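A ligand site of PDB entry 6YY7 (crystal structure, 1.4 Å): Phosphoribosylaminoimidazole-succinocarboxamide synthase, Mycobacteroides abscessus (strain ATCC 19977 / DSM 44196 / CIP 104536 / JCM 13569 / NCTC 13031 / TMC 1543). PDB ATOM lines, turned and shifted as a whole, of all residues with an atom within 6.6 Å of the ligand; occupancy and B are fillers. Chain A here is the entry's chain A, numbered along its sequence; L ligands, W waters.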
ATOM      1  N   HIS A  19      17.446  28.701 -23.334  1.00  0.00           N
ATOM      2  CA  HIS A  19      16.220  29.460 -23.553  1.00  0.00           C
ATOM      3  C   HIS A  19      16.150  29.910 -25.002  1.00  0.00           C
ATOM      4  O   HIS A  19      17.075  30.523 -25.530  1.00  0.00           O
ATOM      5  CB  HIS A  19      16.154  30.660 -22.607  1.00  0.00           C
ATOM      6  CG  HIS A  19      14.984  31.556 -22.852  1.00  0.00           C
ATOM      7  ND1 HIS A  19      15.111  32.823 -23.391  1.00  0.00           N
ATOM      8  CD2 HIS A  19      13.660  31.384 -22.614  1.00  0.00           C
ATOM      9  CE1 HIS A  19      13.915  33.383 -23.478  1.00  0.00           C
ATOM     10  NE2 HIS A  19      13.019  32.531 -23.021  1.00  0.00           N
ATOM     11  N   ALA A  21      12.812  30.979 -26.513  1.00  0.00           N
ATOM     12  CA  ALA A  21      11.675  31.856 -26.735  1.00  0.00           C
ATOM     13  C   ALA A  21      10.955  32.189 -25.445  1.00  0.00           C
ATOM     14  O   ALA A  21      10.860  31.357 -24.532  1.00  0.00           O
ATOM     15  CB  ALA A  21      10.691  31.216 -27.722  1.00  0.00           C
ATOM     16  N   SER A  22      10.473  33.420 -25.372  1.00  0.00           N
ATOM     17  CA  SER A  22       9.637  33.869 -24.272  1.00  0.00           C
ATOM     18  C   SER A  22       8.365  34.494 -24.801  1.00  0.00           C
ATOM     19  O   SER A  22       8.384  35.259 -25.758  1.00  0.00           O
ATOM     20  CB  SER A  22      10.379  34.875 -23.388  1.00  0.00           C
ATOM     21  OG  SER A  22      11.071  34.219 -22.350  1.00  0.00           O
ATOM     22  N   GLY A  23       7.254  34.145 -24.173  1.00  0.00           N
ATOM     23  CA  GLY A  23       5.983  34.774 -24.460  1.00  0.00           C
ATOM     24  C   GLY A  23       5.564  35.570 -23.247  1.00  0.00           C
ATOM     25  O   GLY A  23       6.363  35.795 -22.341  1.00  0.00           O
ATOM     26  N   LYS A  24       4.311  36.012 -23.245  1.00  0.00           N
ATOM     27  CA  LYS A  24       3.771  36.776 -22.130  1.00  0.00           C
ATOM     28  C   LYS A  24       3.817  35.965 -20.829  1.00  0.00           C
ATOM     29  O   LYS A  24       4.209  36.482 -19.775  1.00  0.00           O
ATOM     30  CB  LYS A  24       2.336  37.207 -22.422  1.00  0.00           C
ATOM     31  N   VAL A  25       3.409  34.705 -20.898  1.00  0.00           N
ATOM     32  CA  VAL A  25       3.346  33.890 -19.693  1.00  0.00           C
ATOM     33  C   VAL A  25       3.971  32.509 -19.867  1.00  0.00           C
ATOM     34  O   VAL A  25       4.017  31.730 -18.914  1.00  0.00           O
ATOM     35  CB  VAL A  25       1.879  33.721 -19.184  1.00  0.00           C
ATOM     36  CG1 VAL A  25       1.105  35.029 -19.296  1.00  0.00           C
ATOM     37  CG2 VAL A  25       1.169  32.627 -19.945  1.00  0.00           C
ATOM     38  N   ARG A  26       4.452  32.194 -21.057  1.00  0.00           N
ATOM     39  CA  ARG A  26       5.128  30.926 -21.263  1.00  0.00           C
ATOM     40  C   ARG A  26       6.554  31.087 -21.742  1.00  0.00           C
ATOM     41  O   ARG A  26       6.942  32.144 -22.257  1.00  0.00           O
ATOM     42  CB  ARG A  26       4.340  30.079 -22.254  1.00  0.00           C
ATOM     43  CG  ARG A  26       2.906  29.948 -21.810  1.00  0.00           C
ATOM     44  CD  ARG A  26       2.103  29.394 -22.889  1.00  0.00           C
ATOM     45  NE  ARG A  26       2.153  30.214 -24.090  1.00  0.00           N
ATOM     46  CZ  ARG A  26       1.601  29.835 -25.230  1.00  0.00           C
ATOM     47  NH1 ARG A  26       0.962  28.677 -25.272  1.00  0.00           N
ATOM     48  NH2 ARG A  26       1.667  30.593 -26.317  1.00  0.00           N
ATOM     49  N   GLU A  27       7.343  30.037 -21.548  1.00  0.00           N
ATOM     50  CA  GLU A  27       8.734  30.024 -21.949  1.00  0.00           C
ATOM     51  C   GLU A  27       9.043  28.744 -22.688  1.00  0.00           C
ATOM     52  O   GLU A  27       8.402  27.720 -22.443  1.00  0.00           O
ATOM     53  CB  GLU A  27       9.657  30.133 -20.723  1.00  0.00           C
ATOM     54  CG  GLU A  27       9.531  31.398 -19.927  1.00  0.00           C
ATOM     55  CD  GLU A  27      10.382  31.351 -18.676  1.00  0.00           C
ATOM     56  OE1 GLU A  27      10.732  30.232 -18.237  1.00  0.00           O
ATOM     57  OE2 GLU A  27      10.732  32.427 -18.154  1.00  0.00           O
ATOM     58  N   LEU A  28      10.040  28.793 -23.558  1.00  0.00           N
ATOM     59  CA  LEU A  28      10.422  27.647 -24.363  1.00  0.00           C
ATOM     60  C   LEU A  28      11.927  27.431 -24.281  1.00  0.00           C
ATOM     61  O   LEU A  28      12.698  28.393 -24.450  1.00  0.00           O
ATOM     62  CB  LEU A  28       9.975  27.867 -25.807  1.00  0.00           C
ATOM     63  CG  LEU A  28       9.980  26.682 -26.763  1.00  0.00           C
ATOM     64  CD1 LEU A  28       9.063  25.578 -26.274  1.00  0.00           C
ATOM     65  CD2 LEU A  28       9.536  27.177 -28.134  1.00  0.00           C
ATOM     66  N   LEU A  36      11.976  20.072 -27.100  1.00  0.00           N
ATOM     67  CA  LEU A  36      11.904  21.320 -26.358  1.00  0.00           C
ATOM     68  C   LEU A  36      11.229  21.088 -25.011  1.00  0.00           C
ATOM     69  O   LEU A  36      10.593  20.055 -24.789  1.00  0.00           O
ATOM     70  CB  LEU A  36      11.124  22.370 -27.151  1.00  0.00           C
ATOM     71  CG  LEU A  36      11.547  22.609 -28.599  1.00  0.00           C
ATOM     72  CD1 LEU A  36      10.591  23.574 -29.291  1.00  0.00           C
ATOM     73  CD2 LEU A  36      12.986  23.118 -28.681  1.00  0.00           C
ATOM     74  N   PHE A  38       8.453  22.983 -22.760  1.00  0.00           N
ATOM     75  CA  PHE A  38       7.386  23.968 -22.889  1.00  0.00           C
ATOM     76  C   PHE A  38       6.906  24.321 -21.473  1.00  0.00           C
ATOM     77  O   PHE A  38       6.308  23.481 -20.805  1.00  0.00           O
ATOM     78  CB  PHE A  38       6.253  23.397 -23.745  1.00  0.00           C
ATOM     79  CG  PHE A  38       5.277  24.414 -24.260  1.00  0.00           C
ATOM     80  CD1 PHE A  38       4.213  24.833 -23.487  1.00  0.00           C
ATOM     81  CD2 PHE A  38       5.395  24.903 -25.543  1.00  0.00           C
ATOM     82  CE1 PHE A  38       3.308  25.760 -23.973  1.00  0.00           C
ATOM     83  CE2 PHE A  38       4.502  25.825 -26.034  1.00  0.00           C
ATOM     84  CZ  PHE A  38       3.454  26.252 -25.246  1.00  0.00           C
ATOM     85  N   VAL A  39       7.190  25.545 -21.036  1.00  0.00           N
ATOM     86  CA  VAL A  39       7.007  25.938 -19.646  1.00  0.00           C
ATOM     87  C   VAL A  39       5.918  26.981 -19.455  1.00  0.00           C
ATOM     88  O   VAL A  39       5.952  28.042 -20.083  1.00  0.00           O
ATOM     89  CB  VAL A  39       8.320  26.502 -19.065  1.00  0.00           C
ATOM     90  CG1 VAL A  39       8.140  26.894 -17.599  1.00  0.00           C
ATOM     91  CG2 VAL A  39       9.458  25.492 -19.227  1.00  0.00           C
ATOM     92  N   HIS A  78       2.247  17.299 -29.926  1.00  0.00           N
ATOM     93  CA  HIS A  78       3.692  17.419 -29.789  1.00  0.00           C
ATOM     94  C   HIS A  78       4.248  16.879 -28.480  1.00  0.00           C
ATOM     95  O   HIS A  78       5.457  16.929 -28.272  1.00  0.00           O
ATOM     96  CB  HIS A  78       4.122  18.885 -30.030  1.00  0.00           C
ATOM     97  CG  HIS A  78       3.816  19.858 -28.930  1.00  0.00           C
ATOM     98  ND1 HIS A  78       2.755  19.768 -28.058  1.00  0.00           N
ATOM     99  CD2 HIS A  78       4.398  21.050 -28.681  1.00  0.00           C
ATOM    100  CE1 HIS A  78       2.754  20.827 -27.259  1.00  0.00           C
ATOM    101  NE2 HIS A  78       3.744  21.631 -27.627  1.00  0.00           N
ATOM    102  N   VAL A  99       8.346  18.246 -25.237  1.00  0.00           N
ATOM    103  CA  VAL A  99       7.660  18.195 -26.520  1.00  0.00           C
ATOM    104  C   VAL A  99       8.621  17.970 -27.690  1.00  0.00           C
ATOM    105  O   VAL A  99       9.816  18.250 -27.604  1.00  0.00           O
ATOM    106  CB  VAL A  99       6.831  19.493 -26.772  1.00  0.00           C
ATOM    107  CG1 VAL A  99       5.798  19.685 -25.675  1.00  0.00           C
ATOM    108  CG2 VAL A  99       7.728  20.721 -26.898  1.00  0.00           C
ATOM    109  N   ARG A 100       8.082  17.441 -28.778  1.00  0.00           N
ATOM    110  CA  ARG A 100       8.856  17.242 -30.005  1.00  0.00           C
ATOM    111  C   ARG A 100       9.010  18.560 -30.729  1.00  0.00           C
ATOM    112  O   ARG A 100       8.036  19.302 -30.856  1.00  0.00           O
ATOM    113  CB  ARG A 100       8.171  16.254 -30.950  1.00  0.00           C
ATOM    114  CG  ARG A 100       7.735  14.919 -30.387  1.00  0.00           C
ATOM    115  CD  ARG A 100       7.178  14.051 -31.518  1.00  0.00           C
ATOM    116  NE  ARG A 100       5.716  14.145 -31.653  1.00  0.00           N
ATOM    117  CZ  ARG A 100       5.059  14.003 -32.800  1.00  0.00           C
ATOM    118  NH1 ARG A 100       5.716  13.791 -33.930  1.00  0.00           N
ATOM    119  NH2 ARG A 100       3.730  14.091 -32.826  1.00  0.00           N
ATOM    120  N   ARG A 101      10.202  18.834 -31.248  1.00  0.00           N
ATOM    121  CA  ARG A 101      10.404  20.023 -32.070  1.00  0.00           C
ATOM    122  C   ARG A 101       9.725  19.833 -33.421  1.00  0.00           C
ATOM    123  O   ARG A 101       9.948  18.820 -34.103  1.00  0.00           O
ATOM    124  CB  ARG A 101      11.885  20.323 -32.266  1.00  0.00           C
ATOM    125  CG  ARG A 101      12.112  21.642 -32.989  1.00  0.00           C
ATOM    126  CD  ARG A 101      13.602  21.914 -33.217  1.00  0.00           C
ATOM    127  NE  ARG A 101      14.238  20.819 -33.931  1.00  0.00           N
ATOM    128  CZ  ARG A 101      14.135  20.621 -35.242  1.00  0.00           C
ATOM    129  NH1 ARG A 101      13.415  21.443 -35.989  1.00  0.00           N
ATOM    130  NH2 ARG A 101      14.756  19.591 -35.807  1.00  0.00           N
ATOM    131  N   LEU A 102       8.895  20.803 -33.792  1.00  0.00           N
ATOM    132  CA  LEU A 102       8.192  20.810 -35.078  1.00  0.00           C
ATOM    133  C   LEU A 102       8.586  22.012 -35.920  1.00  0.00           C
ATOM    134  O   LEU A 102       9.081  23.012 -35.402  1.00  0.00           O
ATOM    135  CB  LEU A 102       6.682  20.827 -34.858  1.00  0.00           C
ATOM    136  CG  LEU A 102       6.073  19.723 -34.007  1.00  0.00           C
ATOM    137  CD1 LEU A 102       4.653  20.109 -33.625  1.00  0.00           C
ATOM    138  CD2 LEU A 102       6.090  18.406 -34.779  1.00  0.00           C
ATOM    139  N   ASP A 103       8.334  21.932 -37.220  1.00  0.00           N
ATOM    140  CA  ASP A 103       8.369  23.121 -38.058  1.00  0.00           C
ATOM    141  C   ASP A 103       6.998  23.769 -37.953  1.00  0.00           C
ATOM    142  O   ASP A 103       6.009  23.268 -38.487  1.00  0.00           O
ATOM    143  CB  ASP A 103       8.712  22.782 -39.515  1.00  0.00           C
ATOM    144  CG  ASP A 103      10.142  22.340 -39.693  1.00  0.00           C
ATOM    145  OD1 ASP A 103      11.002  22.717 -38.862  1.00  0.00           O
ATOM    146  OD2 ASP A 103      10.410  21.621 -40.677  1.00  0.00           O
ATOM    147  N   MET A 104       6.928  24.875 -37.243  1.00  0.00           N
ATOM    148  CA  MET A 104       5.644  25.492 -36.926  1.00  0.00           C
ATOM    149  C   MET A 104       5.051  26.199 -38.127  1.00  0.00           C
ATOM    150  O   MET A 104       5.755  26.849 -38.908  1.00  0.00           O
ATOM    151  CB  MET A 104       5.798  26.469 -35.761  1.00  0.00           C
ATOM    152  CG  MET A 104       6.242  25.789 -34.468  1.00  0.00           C
ATOM    153  SD  MET A 104       5.080  24.544 -33.849  1.00  0.00           S
ATOM    154  CE  MET A 104       3.657  25.579 -33.457  1.00  0.00           C
ATOM    155  N   LYS A 154       0.240  36.630 -36.308  1.00  0.00           N
ATOM    156  CA  LYS A 154       0.873  37.470 -35.292  1.00  0.00           C
ATOM    157  C   LYS A 154       1.389  38.766 -35.905  1.00  0.00           C
ATOM    158  O   LYS A 154       1.920  38.770 -37.007  1.00  0.00           O
ATOM    159  CB  LYS A 154       2.025  36.730 -34.604  1.00  0.00           C
ATOM    160  CG  LYS A 154       1.599  35.546 -33.784  1.00  0.00           C
ATOM    161  CD  LYS A 154       2.785  34.952 -33.036  1.00  0.00           C
ATOM    162  CE  LYS A 154       2.358  33.736 -32.222  1.00  0.00           C
ATOM    163  NZ  LYS A 154       1.264  34.059 -31.265  1.00  0.00           N
ATOM    164  N   GLU A 209      -2.025  26.381 -32.310  1.00  0.00           N
ATOM    165  CA  GLU A 209      -0.928  26.391 -33.260  1.00  0.00           C
ATOM    166  C   GLU A 209      -0.573  24.967 -33.641  1.00  0.00           C
ATOM    167  O   GLU A 209      -0.568  24.061 -32.792  1.00  0.00           O
ATOM    168  CB  GLU A 209       0.298  27.101 -32.688  1.00  0.00           C
ATOM    169  CG  GLU A 209       0.167  28.607 -32.649  1.00  0.00           C
ATOM    170  CD  GLU A 209       1.482  29.277 -32.297  1.00  0.00           C
ATOM    171  OE1 GLU A 209       2.247  28.695 -31.500  1.00  0.00           O
ATOM    172  OE2 GLU A 209       1.755  30.379 -32.803  1.00  0.00           O
ATOM    173  N   ALA A 221       0.174  21.543 -31.452  1.00  0.00           N
ATOM    174  CA  ALA A 221       1.265  21.927 -30.567  1.00  0.00           C
ATOM    175  C   ALA A 221       0.804  22.952 -29.530  1.00  0.00           C
ATOM    176  O   ALA A 221      -0.390  23.002 -29.188  1.00  0.00           O
ATOM    177  CB  ALA A 221       2.437  22.454 -31.386  1.00  0.00           C
ATOM    178  N   ASP A 222       1.748  23.742 -29.027  1.00  0.00           N
ATOM    179  CA  ASP A 222       1.471  24.788 -28.063  1.00  0.00           C
ATOM    180  C   ASP A 222       0.661  24.232 -26.877  1.00  0.00           C
ATOM    181  O   ASP A 222       0.972  23.159 -26.352  1.00  0.00           O
ATOM    182  CB  ASP A 222       0.757  25.944 -28.770  1.00  0.00           C
ATOM    183  CG  ASP A 222       0.807  27.248 -28.002  1.00  0.00           C
ATOM    184  OD1 ASP A 222       1.890  27.897 -27.976  1.00  0.00           O
ATOM    185  OD2 ASP A 222      -0.241  27.626 -27.449  1.00  0.00           O
ATOM    186  N   GLU A 223      -0.353  24.961 -26.455  1.00  0.00           N
ATOM    187  CA  GLU A 223      -1.244  24.471 -25.411  1.00  0.00           C
ATOM    188  C   GLU A 223      -2.639  24.431 -25.971  1.00  0.00           C
ATOM    189  O   GLU A 223      -2.975  25.163 -26.912  1.00  0.00           O
ATOM    190  CB  GLU A 223      -1.175  25.350 -24.170  1.00  0.00           C
ATOM    191  CG  GLU A 223      -1.884  26.690 -24.294  1.00  0.00           C
ATOM    192  CD  GLU A 223      -1.475  27.644 -23.202  1.00  0.00           C
ATOM    193  OE1 GLU A 223      -2.307  28.457 -22.751  1.00  0.00           O
ATOM    194  OE2 GLU A 223      -0.296  27.587 -22.797  1.00  0.00           O
HETATM  195  C1  LIG L   1       7.381  25.396 -31.130  1.00  0.00           C
HETATM  196  C2  LIG L   1       8.830  24.020 -32.313  1.00  0.00           C
HETATM  197  O1  LIG L   1       6.104  28.632 -27.355  1.00  0.00           O
HETATM  198  C3  LIG L   1       5.595  29.592 -27.919  1.00  0.00           C
HETATM  199  O2  LIG L   1       5.537  30.815 -27.245  1.00  0.00           O
HETATM  200  C4  LIG L   1       5.734  30.668 -25.859  1.00  0.00           C
HETATM  201  C5  LIG L   1       7.148  31.087 -25.528  1.00  0.00           C
HETATM  202  C6  LIG L   1       5.052  29.434 -29.311  1.00  0.00           C
HETATM  203  N1  LIG L   1       5.990  28.577 -29.976  1.00  0.00           N
HETATM  204  C7  LIG L   1       5.890  27.252 -30.057  1.00  0.00           C
HETATM  205  C8  LIG L   1       6.994  26.817 -30.768  1.00  0.00           C
HETATM  206  C9  LIG L   1       6.742  24.232 -30.587  1.00  0.00           C
HETATM  207  C10 LIG L   1       5.558  24.313 -29.626  1.00  0.00           C
HETATM  208  N2  LIG L   1       4.684  24.359 -28.903  1.00  0.00           N
HETATM  209  C11 LIG L   1       7.221  22.966 -31.005  1.00  0.00           C
HETATM  210  N3  LIG L   1       6.637  21.752 -30.520  1.00  0.00           N
HETATM  211  N4  LIG L   1       8.257  22.900 -31.860  1.00  0.00           N
HETATM  212  N5  LIG L   1       8.409  25.226 -31.954  1.00  0.00           N
HETATM  213  C12 LIG L   1       7.757  27.933 -31.092  1.00  0.00           C
HETATM  214  N6  LIG L   1       7.112  29.019 -30.593  1.00  0.00           N
HETATM  215  O   HOH W   1       9.547  27.090 -33.727  1.00  0.00           O
HETATM  216  O   HOH W   2       8.372  31.680 -30.837  1.00  0.00           O
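O of Arg 100 is in hydrogen-bond range of N3 of the ligand. The backbone NH (N) of Leu 102 sits at hydrogen-bond distance from a nitrogen (N4) of the ligand. NE2 of His 78 lies within hydrogen-bond range of N2 of the ligand, 3.2 Å away. The backbone NH of Asp 222 is in hydrogen-bond range of a nitrogen (N2) of the ligand, at 3.0 Å.
Ala 21 touches the ligand. Ser 22 touches the ligand. Gly 23 touches the ligand (N to C5, 3.3 Å). Arg 26 touches the ligand (O to C5, 3.4 Å). Leu 28 touches the ligand (CD2 to C12, 3.5 Å). CD1 of Leu 36 touches C2 of the ligand, 3.5 Å away. Phe 38 touches the ligand (CE2 to N2, 3.2 Å). Val 99 touches the ligand (CG2 to N3, 3.9 Å). Arg 101 touches the ligand (CA to N4, 3.6 Å). Met 104 touches the ligand (CG to N5, 3.4 Å). OE1 of Glu 209 touches C6 of the ligand, 3.6 Å away. CB of Ala 221 touches N2 of the ligand, 3.9 Å away. Of the 24 residues printed, 16 come within 4 Å of the ligand. The nearest printed residue that does not touch the ligand is Glu 27 (4.1 Å).
The backbone NH (N) of Arg 100 is in hydrogen-bond range of the backbone carbonyl oxygen (O) of His 78, at 2.7 Å. A ring nitrogen (NE2) of His 78 sits at hydrogen-bond distance from the backbone NH of Asp 222. The side-chain carboxylate (OD2) of Asp 222 is in salt-bridge range of the guanidinium group (NH1) of Arg 26. The side-chain carboxylate of Glu 223 lies within salt-bridge range of the guanidinium group of Arg 26 (3.0 Å). N of Leu 36 lies within hydrogen-bond range of O of Val 99 (2.9 Å). The backbone carbonyl oxygen (O) of Ala 21 lies within hydrogen-bond range of the backbone NH (N) of Leu 28. The guanidinium group of Arg 101 is in salt-bridge range of the side-chain carboxylate of Asp 103, at 3.96 Å. The backbone carbonyl oxygen (O) of Ala 21 lies within hydrogen-bond range of a ring nitrogen (NE2) of His 19.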
